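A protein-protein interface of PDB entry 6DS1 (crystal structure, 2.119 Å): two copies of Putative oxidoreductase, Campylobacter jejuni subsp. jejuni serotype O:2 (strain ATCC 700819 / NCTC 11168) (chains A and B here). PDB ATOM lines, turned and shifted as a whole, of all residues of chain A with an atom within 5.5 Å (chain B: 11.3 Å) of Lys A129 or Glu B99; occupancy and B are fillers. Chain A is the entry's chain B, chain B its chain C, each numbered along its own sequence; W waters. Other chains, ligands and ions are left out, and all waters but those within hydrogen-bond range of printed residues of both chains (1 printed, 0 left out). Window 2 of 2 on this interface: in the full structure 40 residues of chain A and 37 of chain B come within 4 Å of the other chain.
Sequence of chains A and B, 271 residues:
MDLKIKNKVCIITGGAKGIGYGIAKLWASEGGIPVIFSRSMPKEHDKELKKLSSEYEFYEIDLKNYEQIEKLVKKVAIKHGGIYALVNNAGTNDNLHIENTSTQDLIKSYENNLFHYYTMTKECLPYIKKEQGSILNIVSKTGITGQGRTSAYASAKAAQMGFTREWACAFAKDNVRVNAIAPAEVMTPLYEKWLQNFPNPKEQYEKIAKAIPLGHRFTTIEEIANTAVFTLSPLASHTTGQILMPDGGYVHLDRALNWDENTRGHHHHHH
OH of Tyr A118 is in hydrogen-bond range of O of Thr B101 (2.7 Å).
The side-chain amino group (NZ) of Lys A122 sits at hydrogen-bond distance from the backbone carbonyl oxygen (O) of Glu B99, at 3.5 Å.
The side-chain amino group (NZ) of Lys A122 is in hydrogen-bond range of the backbone carbonyl oxygen (O) of Thr B101 (3.2 Å).
The side-chain hydroxyl (OH) of Tyr A118 sits close to the backbone carbonyl oxygen (O) of Ile B98, 3.4 Å away.
The side-chain amino group (NZ) of Lys A129 is in salt-bridge range of the side-chain carboxylate (OE2) of Glu B99, at 2.5 Å.
The side-chain amino group of Lys A122 sits at hydrogen-bond distance from the backbone carbonyl oxygen of Ile B98.
The side-chain carboxylate (OE1) of Glu B99 is in hydrogen-bond range of a ring nitrogen (NE2) of His B97 (2.9 Å).
OG1 of Thr B101 lies within hydrogen-bond range of O of His B97.
The backbone carbonyl oxygen (O) of His B97 sits close to the side-chain amide oxygen (OD1) of Asn B100 (3.4 Å).
ND1 of His B97 is in hydrogen-bond range of O of Gly B148, at 3.4 Å.
The backbone carbonyl oxygen (O) of Phe A171 is in hydrogen-bond range of the backbone NH (N) of Val A176 (3.0 Å).
Among the printed residues, pairs that only touch across the chains: Phe A171 with Glu B99 (3.6 Å), Tyr A118 with Thr B103 (3.7 Å), Tyr A118 with Leu B106 (3.7 Å), Phe A171 with Ile B98 (3.7 Å), Leu A125 with Ile B98 (3.8 Å) and Tyr A118 with His B97 (3.95 Å).
Of chain A, only Lys A122, Lys A129 and Phe A171 come within 4 Å of Glu B99.
Of the printed residues of chain B, Lys A122 touches Ile B98, Glu B99 and Thr B101.
Of chain B, only Ile B98 comes within 4 Å of Leu A125.
No residue of chain B comes within 4 Å of Ile A128.
No residue of chain B comes within 4 Å of Gln A132.
No residue of chain B comes within 4 Å of Gly A133.
Printed residues of chain A within 4 Å of His B97: Tyr A118.
Of the printed residues of chain A, Ile B98 touches Tyr A118, Lys A122, Leu A125 and Phe A171.
Of the printed residues of chain A, Thr B101 touches Tyr A118 (2.7 Å) and Lys A122 (3.2 Å).
Printed residues of chain B within 4 Å of Phe A171: Ile B98 and Glu B99.
The nearest printed residue of chain B that does not touch Phe A171 is His B97 (4.1 Å).
Of the 15 printed residues of chain A, 5 touch a printed residue of chain B.
Hydrophobic or aromatic side chains of chain A within 4 Å of the printed part of chain B: Tyr A118, Leu A125 and Phe A171.
Along chain A the printed residues that touch a printed residue of chain B span positions 118 to 171.
Among the printed residues, 12 pairs touch across the chains.
Among the printed residues, Asp or Glu carboxylates within 4 Å of a Lys or Arg side-chain nitrogen of the other chain: Lys A129 with Glu B99 (2.5 Å).
No position is printed for both chains.
Of the 12 pairs that touch across the chains among the printed residues, none has its exchanged pair printed and touching as well.
Water W1 lies within hydrogen-bond range of the side-chain amino group of Lys A122 (3.2 Å) and the backbone carbonyl oxygen of Glu B99 (3.5 Å).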
ATOM      1  N   TYR A 118     -28.871  15.075  19.274  1.00  0.00           N
ATOM      2  CA  TYR A 118     -28.398  13.709  19.076  1.00  0.00           C
ATOM      3  C   TYR A 118     -28.040  13.460  17.618  1.00  0.00           C
ATOM      4  O   TYR A 118     -26.946  12.958  17.309  1.00  0.00           O
ATOM      5  CB  TYR A 118     -29.477  12.718  19.547  1.00  0.00           C
ATOM      6  CG  TYR A 118     -29.146  11.257  19.295  1.00  0.00           C
ATOM      7  CD1 TYR A 118     -28.536  10.489  20.276  1.00  0.00           C
ATOM      8  CD2 TYR A 118     -29.436  10.649  18.070  1.00  0.00           C
ATOM      9  CE1 TYR A 118     -28.224   9.158  20.059  1.00  0.00           C
ATOM     10  CE2 TYR A 118     -29.129   9.313  17.842  1.00  0.00           C
ATOM     11  CZ  TYR A 118     -28.521   8.574  18.852  1.00  0.00           C
ATOM     12  OH  TYR A 118     -28.203   7.246  18.656  1.00  0.00           O
ATOM     13  N   LYS A 122     -24.460  12.659  16.031  1.00  0.00           N
ATOM     14  CA  LYS A 122     -24.316  11.386  15.336  1.00  0.00           C
ATOM     15  C   LYS A 122     -23.673  11.569  13.972  1.00  0.00           C
ATOM     16  O   LYS A 122     -22.686  10.909  13.649  1.00  0.00           O
ATOM     17  CB  LYS A 122     -25.689  10.713  15.198  1.00  0.00           C
ATOM     18  CG  LYS A 122     -25.642   9.308  14.616  1.00  0.00           C
ATOM     19  CD  LYS A 122     -27.026   8.775  14.358  1.00  0.00           C
ATOM     20  CE  LYS A 122     -26.991   7.476  13.549  1.00  0.00           C
ATOM     21  NZ  LYS A 122     -26.138   6.452  14.196  1.00  0.00           N
ATOM     22  N   CYS A 124     -22.060  14.239  12.696  1.00  0.00           N
ATOM     23  CA  CYS A 124     -20.777  14.940  12.692  1.00  0.00           C
ATOM     24  C   CYS A 124     -19.642  14.084  13.264  1.00  0.00           C
ATOM     25  O   CYS A 124     -18.473  14.299  12.914  1.00  0.00           O
ATOM     26  CB  CYS A 124     -20.894  16.252  13.477  1.00  0.00           C
ATOM     27  SG  CYS A 124     -21.857  17.534  12.620  1.00  0.00           S
ATOM     28  N   LEU A 125     -19.966  13.118  14.134  1.00  0.00           N
ATOM     29  CA  LEU A 125     -18.939  12.370  14.861  1.00  0.00           C
ATOM     30  C   LEU A 125     -17.847  11.786  13.969  1.00  0.00           C
ATOM     31  O   LEU A 125     -16.663  11.969  14.296  1.00  0.00           O
ATOM     32  CB  LEU A 125     -19.600  11.266  15.702  1.00  0.00           C
ATOM     33  CG  LEU A 125     -19.894  11.705  17.143  1.00  0.00           C
ATOM     34  CD1 LEU A 125     -20.886  10.787  17.823  1.00  0.00           C
ATOM     35  CD2 LEU A 125     -18.624  11.823  17.972  1.00  0.00           C
ATOM     36  N   PRO A 126     -18.144  11.100  12.853  1.00  0.00           N
ATOM     37  CA  PRO A 126     -17.036  10.524  12.055  1.00  0.00           C
ATOM     38  C   PRO A 126     -16.004  11.556  11.643  1.00  0.00           C
ATOM     39  O   PRO A 126     -14.798  11.277  11.692  1.00  0.00           O
ATOM     40  CB  PRO A 126     -17.747   9.915  10.839  1.00  0.00           C
ATOM     41  CG  PRO A 126     -19.171   9.685  11.302  1.00  0.00           C
ATOM     42  CD  PRO A 126     -19.467  10.793  12.262  1.00  0.00           C
ATOM     43  N   TYR A 127     -16.451  12.766  11.291  1.00  0.00           N
ATOM     44  CA  TYR A 127     -15.540  13.842  10.897  1.00  0.00           C
ATOM     45  C   TYR A 127     -14.838  14.489  12.085  1.00  0.00           C
ATOM     46  O   TYR A 127     -13.659  14.847  11.989  1.00  0.00           O
ATOM     47  CB  TYR A 127     -16.301  14.906  10.109  1.00  0.00           C
ATOM     48  CG  TYR A 127     -17.064  14.314   8.961  1.00  0.00           C
ATOM     49  CD1 TYR A 127     -16.406  13.942   7.792  1.00  0.00           C
ATOM     50  CD2 TYR A 127     -18.439  14.093   9.052  1.00  0.00           C
ATOM     51  CE1 TYR A 127     -17.093  13.374   6.736  1.00  0.00           C
ATOM     52  CE2 TYR A 127     -19.139  13.525   8.001  1.00  0.00           C
ATOM     53  CZ  TYR A 127     -18.461  13.179   6.843  1.00  0.00           C
ATOM     54  OH  TYR A 127     -19.148  12.629   5.807  1.00  0.00           O
ATOM     55  N   ILE A 128     -15.549  14.692  13.197  1.00  0.00           N
ATOM     56  CA  ILE A 128     -14.910  15.340  14.334  1.00  0.00           C
ATOM     57  C   ILE A 128     -13.895  14.399  14.966  1.00  0.00           C
ATOM     58  O   ILE A 128     -12.849  14.843  15.461  1.00  0.00           O
ATOM     59  CB  ILE A 128     -15.969  15.842  15.338  1.00  0.00           C
ATOM     60  CG1 ILE A 128     -16.836  16.935  14.688  1.00  0.00           C
ATOM     61  CG2 ILE A 128     -15.303  16.370  16.603  1.00  0.00           C
ATOM     62  CD1 ILE A 128     -18.021  17.433  15.548  1.00  0.00           C
ATOM     63  N   LYS A 129     -14.154  13.090  14.924  1.00  0.00           N
ATOM     64  CA  LYS A 129     -13.182  12.131  15.444  1.00  0.00           C
ATOM     65  C   LYS A 129     -11.909  12.132  14.610  1.00  0.00           C
ATOM     66  O   LYS A 129     -10.808  11.990  15.153  1.00  0.00           O
ATOM     67  CB  LYS A 129     -13.791  10.731  15.495  1.00  0.00           C
ATOM     68  CG  LYS A 129     -14.795  10.572  16.632  1.00  0.00           C
ATOM     69  CD  LYS A 129     -15.705   9.370  16.407  1.00  0.00           C
ATOM     70  CE  LYS A 129     -14.955   8.081  16.661  1.00  0.00           C
ATOM     71  NZ  LYS A 129     -15.668   6.917  16.099  1.00  0.00           N
ATOM     72  N   LYS A 130     -12.039  12.312  13.294  1.00  0.00           N
ATOM     73  CA  LYS A 130     -10.862  12.331  12.436  1.00  0.00           C
ATOM     74  C   LYS A 130      -9.968  13.517  12.769  1.00  0.00           C
ATOM     75  O   LYS A 130      -8.738  13.405  12.734  1.00  0.00           O
ATOM     76  CB  LYS A 130     -11.284  12.355  10.961  1.00  0.00           C
ATOM     77  CG  LYS A 130     -10.112  12.290   9.968  1.00  0.00           C
ATOM     78  CD  LYS A 130     -10.109  13.501   9.030  1.00  0.00           C
ATOM     79  CE  LYS A 130      -8.897  13.530   8.089  1.00  0.00           C
ATOM     80  NZ  LYS A 130      -8.741  14.849   7.388  1.00  0.00           N
ATOM     81  N   GLU A 131     -10.566  14.657  13.122  1.00  0.00           N
ATOM     82  CA  GLU A 131      -9.820  15.862  13.460  1.00  0.00           C
ATOM     83  C   GLU A 131      -9.631  16.054  14.965  1.00  0.00           C
ATOM     84  O   GLU A 131      -9.203  17.133  15.386  1.00  0.00           O
ATOM     85  CB  GLU A 131     -10.517  17.082  12.856  1.00  0.00           C
ATOM     86  CG  GLU A 131     -10.633  16.987  11.341  1.00  0.00           C
ATOM     87  CD  GLU A 131     -11.118  18.264  10.692  1.00  0.00           C
ATOM     88  OE1 GLU A 131     -11.035  19.345  11.328  1.00  0.00           O
ATOM     89  OE2 GLU A 131     -11.577  18.185   9.531  1.00  0.00           O
ATOM     90  N   GLN A 132      -9.926  15.039  15.771  1.00  0.00           N
ATOM     91  CA  GLN A 132      -9.807  15.105  17.232  1.00  0.00           C
ATOM     92  C   GLN A 132     -10.367  16.429  17.759  1.00  0.00           C
ATOM     93  O   GLN A 132      -9.700  17.208  18.442  1.00  0.00           O
ATOM     94  CB  GLN A 132      -8.357  14.882  17.665  1.00  0.00           C
ATOM     95  CG  GLN A 132      -7.866  13.479  17.350  1.00  0.00           C
ATOM     96  CD  GLN A 132      -6.421  13.225  17.745  1.00  0.00           C
ATOM     97  OE1 GLN A 132      -5.939  13.728  18.758  1.00  0.00           O
ATOM     98  NE2 GLN A 132      -5.728  12.433  16.940  1.00  0.00           N
ATOM     99  N   GLY A 133     -11.623  16.668  17.405  1.00  0.00           N
ATOM    100  CA  GLY A 133     -12.242  17.962  17.525  1.00  0.00           C
ATOM    101  C   GLY A 133     -13.052  18.125  18.791  1.00  0.00           C
ATOM    102  O   GLY A 133     -12.735  17.552  19.843  1.00  0.00           O
ATOM    103  N   PHE A 171     -15.989   9.325  23.828  1.00  0.00           N
ATOM    104  CA  PHE A 171     -14.983   9.729  22.848  1.00  0.00           C
ATOM    105  C   PHE A 171     -13.707  10.302  23.453  1.00  0.00           C
ATOM    106  O   PHE A 171     -12.867  10.835  22.708  1.00  0.00           O
ATOM    107  CB  PHE A 171     -15.626  10.719  21.869  1.00  0.00           C
ATOM    108  CG  PHE A 171     -16.937  10.227  21.344  1.00  0.00           C
ATOM    109  CD1 PHE A 171     -16.990   9.030  20.635  1.00  0.00           C
ATOM    110  CD2 PHE A 171     -18.114  10.912  21.598  1.00  0.00           C
ATOM    111  CE1 PHE A 171     -18.194   8.537  20.163  1.00  0.00           C
ATOM    112  CE2 PHE A 171     -19.325  10.424  21.137  1.00  0.00           C
ATOM    113  CZ  PHE A 171     -19.365   9.235  20.425  1.00  0.00           C
ATOM    114  N   ASP A 174     -10.903   8.827  21.824  1.00  0.00           N
ATOM    115  CA  ASP A 174     -10.656   9.385  20.496  1.00  0.00           C
ATOM    116  C   ASP A 174     -10.087  10.787  20.545  1.00  0.00           C
ATOM    117  O   ASP A 174      -9.906  11.405  19.488  1.00  0.00           O
ATOM    118  CB  ASP A 174     -11.944   9.406  19.672  1.00  0.00           C
ATOM    119  CG  ASP A 174     -12.480   8.017  19.408  1.00  0.00           C
ATOM    120  OD1 ASP A 174     -11.936   7.327  18.520  1.00  0.00           O
ATOM    121  OD2 ASP A 174     -13.419   7.610  20.105  1.00  0.00           O
ATOM    122  N   VAL A 176     -11.699  13.355  21.494  1.00  0.00           N
ATOM    123  CA  VAL A 176     -12.768  14.296  21.173  1.00  0.00           C
ATOM    124  C   VAL A 176     -13.299  14.840  22.493  1.00  0.00           C
ATOM    125  O   VAL A 176     -13.691  14.072  23.380  1.00  0.00           O
ATOM    126  CB  VAL A 176     -13.878  13.647  20.332  1.00  0.00           C
ATOM    127  CG1 VAL A 176     -15.066  14.590  20.200  1.00  0.00           C
ATOM    128  CG2 VAL A 176     -13.348  13.308  18.943  1.00  0.00           C
ATOM    129  N   ASN B  95     -28.609   0.291  26.460  1.00  0.00           N
ATOM    130  CA  ASN B  95     -27.255   0.318  25.888  1.00  0.00           C
ATOM    131  C   ASN B  95     -27.274   0.636  24.395  1.00  0.00           C
ATOM    132  O   ASN B  95     -26.693  -0.072  23.567  1.00  0.00           O
ATOM    133  CB  ASN B  95     -26.537  -1.000  26.149  1.00  0.00           C
ATOM    134  CG  ASN B  95     -26.199  -1.184  27.604  1.00  0.00           C
ATOM    135  OD1 ASN B  95     -26.702  -2.097  28.256  1.00  0.00           O
ATOM    136  ND2 ASN B  95     -25.350  -0.300  28.132  1.00  0.00           N
ATOM    137  N   LEU B  96     -27.969   1.707  24.054  1.00  0.00           N
ATOM    138  CA  LEU B  96     -28.055   2.186  22.682  1.00  0.00           C
ATOM    139  C   LEU B  96     -26.999   3.271  22.517  1.00  0.00           C
ATOM    140  O   LEU B  96     -27.125   4.361  23.082  1.00  0.00           O
ATOM    141  CB  LEU B  96     -29.460   2.698  22.367  1.00  0.00           C
ATOM    142  CG  LEU B  96     -30.549   1.638  22.586  1.00  0.00           C
ATOM    143  CD1 LEU B  96     -31.945   2.258  22.560  1.00  0.00           C
ATOM    144  CD2 LEU B  96     -30.426   0.469  21.564  1.00  0.00           C
ATOM    145  N   HIS B  97     -25.941   2.950  21.784  1.00  0.00           N
ATOM    146  CA  HIS B  97     -24.828   3.857  21.569  1.00  0.00           C
ATOM    147  C   HIS B  97     -25.100   4.707  20.329  1.00  0.00           C
ATOM    148  O   HIS B  97     -25.730   4.251  19.376  1.00  0.00           O
ATOM    149  CB  HIS B  97     -23.531   3.053  21.430  1.00  0.00           C
ATOM    150  CG  HIS B  97     -22.334   3.886  21.100  1.00  0.00           C
ATOM    151  ND1 HIS B  97     -21.981   5.003  21.829  1.00  0.00           N
ATOM    152  CD2 HIS B  97     -21.403   3.758  20.125  1.00  0.00           C
ATOM    153  CE1 HIS B  97     -20.891   5.537  21.308  1.00  0.00           C
ATOM    154  NE2 HIS B  97     -20.520   4.803  20.273  1.00  0.00           N
ATOM    155  N   ILE B  98     -24.643   5.964  20.366  1.00  0.00           N
ATOM    156  CA  ILE B  98     -25.025   6.926  19.335  1.00  0.00           C
ATOM    157  C   ILE B  98     -24.568   6.456  17.956  1.00  0.00           C
ATOM    158  O   ILE B  98     -25.302   6.573  16.969  1.00  0.00           O
ATOM    159  CB  ILE B  98     -24.475   8.329  19.677  1.00  0.00           C
ATOM    160  CG1 ILE B  98     -24.863   9.357  18.603  1.00  0.00           C
ATOM    161  CG2 ILE B  98     -22.957   8.316  19.865  1.00  0.00           C
ATOM    162  CD1 ILE B  98     -24.816  10.844  19.101  1.00  0.00           C
ATOM    163  N   GLU B  99     -23.367   5.884  17.868  1.00  0.00           N
ATOM    164  CA  GLU B  99     -22.777   5.631  16.558  1.00  0.00           C
ATOM    165  C   GLU B  99     -23.473   4.504  15.797  1.00  0.00           C
ATOM    166  O   GLU B  99     -23.328   4.429  14.574  1.00  0.00           O
ATOM    167  CB  GLU B  99     -21.273   5.361  16.703  1.00  0.00           C
ATOM    168  CG  GLU B  99     -20.461   6.643  16.991  1.00  0.00           C
ATOM    169  CD  GLU B  99     -18.973   6.380  17.219  1.00  0.00           C
ATOM    170  OE1 GLU B  99     -18.639   5.611  18.152  1.00  0.00           O
ATOM    171  OE2 GLU B  99     -18.143   6.931  16.448  1.00  0.00           O
ATOM    172  N   ASN B 100     -24.261   3.655  16.464  1.00  0.00           N
ATOM    173  CA  ASN B 100     -25.037   2.664  15.724  1.00  0.00           C
ATOM    174  C   ASN B 100     -26.499   2.607  16.163  1.00  0.00           C
ATOM    175  O   ASN B 100     -27.161   1.582  15.949  1.00  0.00           O
ATOM    176  CB  ASN B 100     -24.390   1.278  15.821  1.00  0.00           C
ATOM    177  CG  ASN B 100     -24.029   0.899  17.232  1.00  0.00           C
ATOM    178  OD1 ASN B 100     -24.696   1.290  18.190  1.00  0.00           O
ATOM    179  ND2 ASN B 100     -22.959   0.137  17.372  1.00  0.00           N
ATOM    180  N   THR B 101     -27.039   3.682  16.742  1.00  0.00           N
ATOM    181  CA  THR B 101     -28.471   3.756  17.022  1.00  0.00           C
ATOM    182  C   THR B 101     -29.078   4.929  16.266  1.00  0.00           C
ATOM    183  O   THR B 101     -28.553   6.050  16.310  1.00  0.00           O
ATOM    184  CB  THR B 101     -28.752   3.884  18.523  1.00  0.00           C
ATOM    185  OG1 THR B 101     -28.012   2.889  19.233  1.00  0.00           O
ATOM    186  CG2 THR B 101     -30.225   3.678  18.806  1.00  0.00           C
ATOM    187  N   SER B 102     -30.164   4.668  15.551  1.00  0.00           N
ATOM    188  CA  SER B 102     -30.793   5.746  14.820  1.00  0.00           C
ATOM    189  C   SER B 102     -31.494   6.691  15.792  1.00  0.00           C
ATOM    190  O   SER B 102     -31.729   6.373  16.966  1.00  0.00           O
ATOM    191  CB  SER B 102     -31.796   5.200  13.809  1.00  0.00           C
ATOM    192  OG  SER B 102     -32.887   4.584  14.474  1.00  0.00           O
ATOM    193  N   THR B 103     -31.835   7.875  15.286  1.00  0.00           N
ATOM    194  CA  THR B 103     -32.680   8.775  16.063  1.00  0.00           C
ATOM    195  C   THR B 103     -34.041   8.138  16.346  1.00  0.00           C
ATOM    196  O   THR B 103     -34.587   8.298  17.438  1.00  0.00           O
ATOM    197  CB  THR B 103     -32.830  10.111  15.329  1.00  0.00           C
ATOM    198  OG1 THR B 103     -31.530  10.656  15.064  1.00  0.00           O
ATOM    199  CG2 THR B 103     -33.627  11.114  16.168  1.00  0.00           C
ATOM    200  N   ASP B 105     -34.756   4.979  16.844  1.00  0.00           N
ATOM    201  CA  ASP B 105     -34.620   4.069  17.977  1.00  0.00           C
ATOM    202  C   ASP B 105     -34.317   4.809  19.279  1.00  0.00           C
ATOM    203  O   ASP B 105     -34.713   4.339  20.350  1.00  0.00           O
ATOM    204  CB  ASP B 105     -33.543   3.018  17.685  1.00  0.00           C
ATOM    205  CG  ASP B 105     -33.996   1.992  16.645  1.00  0.00           C
ATOM    206  OD1 ASP B 105     -35.202   1.967  16.313  1.00  0.00           O
ATOM    207  OD2 ASP B 105     -33.143   1.222  16.154  1.00  0.00           O
ATOM    208  N   LEU B 106     -33.640   5.962  19.223  1.00  0.00           N
ATOM    209  CA  LEU B 106     -33.559   6.815  20.411  1.00  0.00           C
ATOM    210  C   LEU B 106     -34.952   7.176  20.914  1.00  0.00           C
ATOM    211  O   LEU B 106     -35.262   7.010  22.099  1.00  0.00           O
ATOM    212  CB  LEU B 106     -32.768   8.090  20.109  1.00  0.00           C
ATOM    213  CG  LEU B 106     -32.819   9.181  21.188  1.00  0.00           C
ATOM    214  CD1 LEU B 106     -31.859   8.880  22.349  1.00  0.00           C
ATOM    215  CD2 LEU B 106     -32.514  10.546  20.582  1.00  0.00           C
ATOM    216  N   GLY B 148     -20.845   5.748  28.339  1.00  0.00           N
ATOM    217  CA  GLY B 148     -20.095   5.713  27.094  1.00  0.00           C
ATOM    218  C   GLY B 148     -20.694   4.919  25.947  1.00  0.00           C
ATOM    219  O   GLY B 148     -20.401   5.190  24.779  1.00  0.00           O
ATOM    220  N   ARG B 149     -21.546   3.941  26.249  1.00  0.00           N
ATOM    221  CA  ARG B 149     -22.162   3.140  25.196  1.00  0.00           C
ATOM    222  C   ARG B 149     -23.676   3.113  25.341  1.00  0.00           C
ATOM    223  O   ARG B 149     -24.328   2.162  24.904  1.00  0.00           O
ATOM    224  CB  ARG B 149     -21.609   1.714  25.196  1.00  0.00           C
ATOM    225  CG  ARG B 149     -20.202   1.592  24.611  1.00  0.00           C
ATOM    226  CD  ARG B 149     -20.128   2.263  23.257  1.00  0.00           C
ATOM    227  NE  ARG B 149     -18.803   2.200  22.646  1.00  0.00           N
ATOM    228  CZ  ARG B 149     -17.916   3.193  22.656  1.00  0.00           C
ATOM    229  NH1 ARG B 149     -18.200   4.342  23.262  1.00  0.00           N
ATOM    230  NH2 ARG B 149     -16.738   3.035  22.060  1.00  0.00           N
ATOM    231  N   THR B 150     -24.255   4.139  25.952  1.00  0.00           N
ATOM    232  CA  THR B 150     -25.682   4.101  26.261  1.00  0.00           C
ATOM    233  C   THR B 150     -26.284   5.517  26.242  1.00  0.00           C
ATOM    234  O   THR B 150     -26.765   6.064  27.241  1.00  0.00           O
ATOM    235  CB  THR B 150     -25.852   3.336  27.576  1.00  0.00           C
ATOM    236  OG1 THR B 150     -27.226   2.984  27.774  1.00  0.00           O
ATOM    237  CG2 THR B 150     -25.279   4.118  28.792  1.00  0.00           C
ATOM    238  N   SER B 151     -26.273   6.141  25.056  1.00  0.00           N
ATOM    239  CA  SER B 151     -26.702   7.535  24.914  1.00  0.00           C
ATOM    240  C   SER B 151     -28.180   7.728  25.257  1.00  0.00           C
ATOM    241  O   SER B 151     -28.559   8.769  25.810  1.00  0.00           O
ATOM    242  CB  SER B 151     -26.436   8.037  23.488  1.00  0.00           C
ATOM    243  OG  SER B 151     -25.087   8.435  23.280  1.00  0.00           O
ATOM    244  N   ALA B 152     -29.039   6.764  24.891  1.00  0.00           N
ATOM    245  CA  ALA B 152     -30.478   6.940  25.103  1.00  0.00           C
ATOM    246  C   ALA B 152     -30.825   6.884  26.580  1.00  0.00           C
ATOM    247  O   ALA B 152     -31.652   7.667  27.062  1.00  0.00           O
ATOM    248  CB  ALA B 152     -31.263   5.872  24.342  1.00  0.00           C
HETATM  249  O   HOH W   1     -23.440   7.243  12.578  1.00  0.00           O
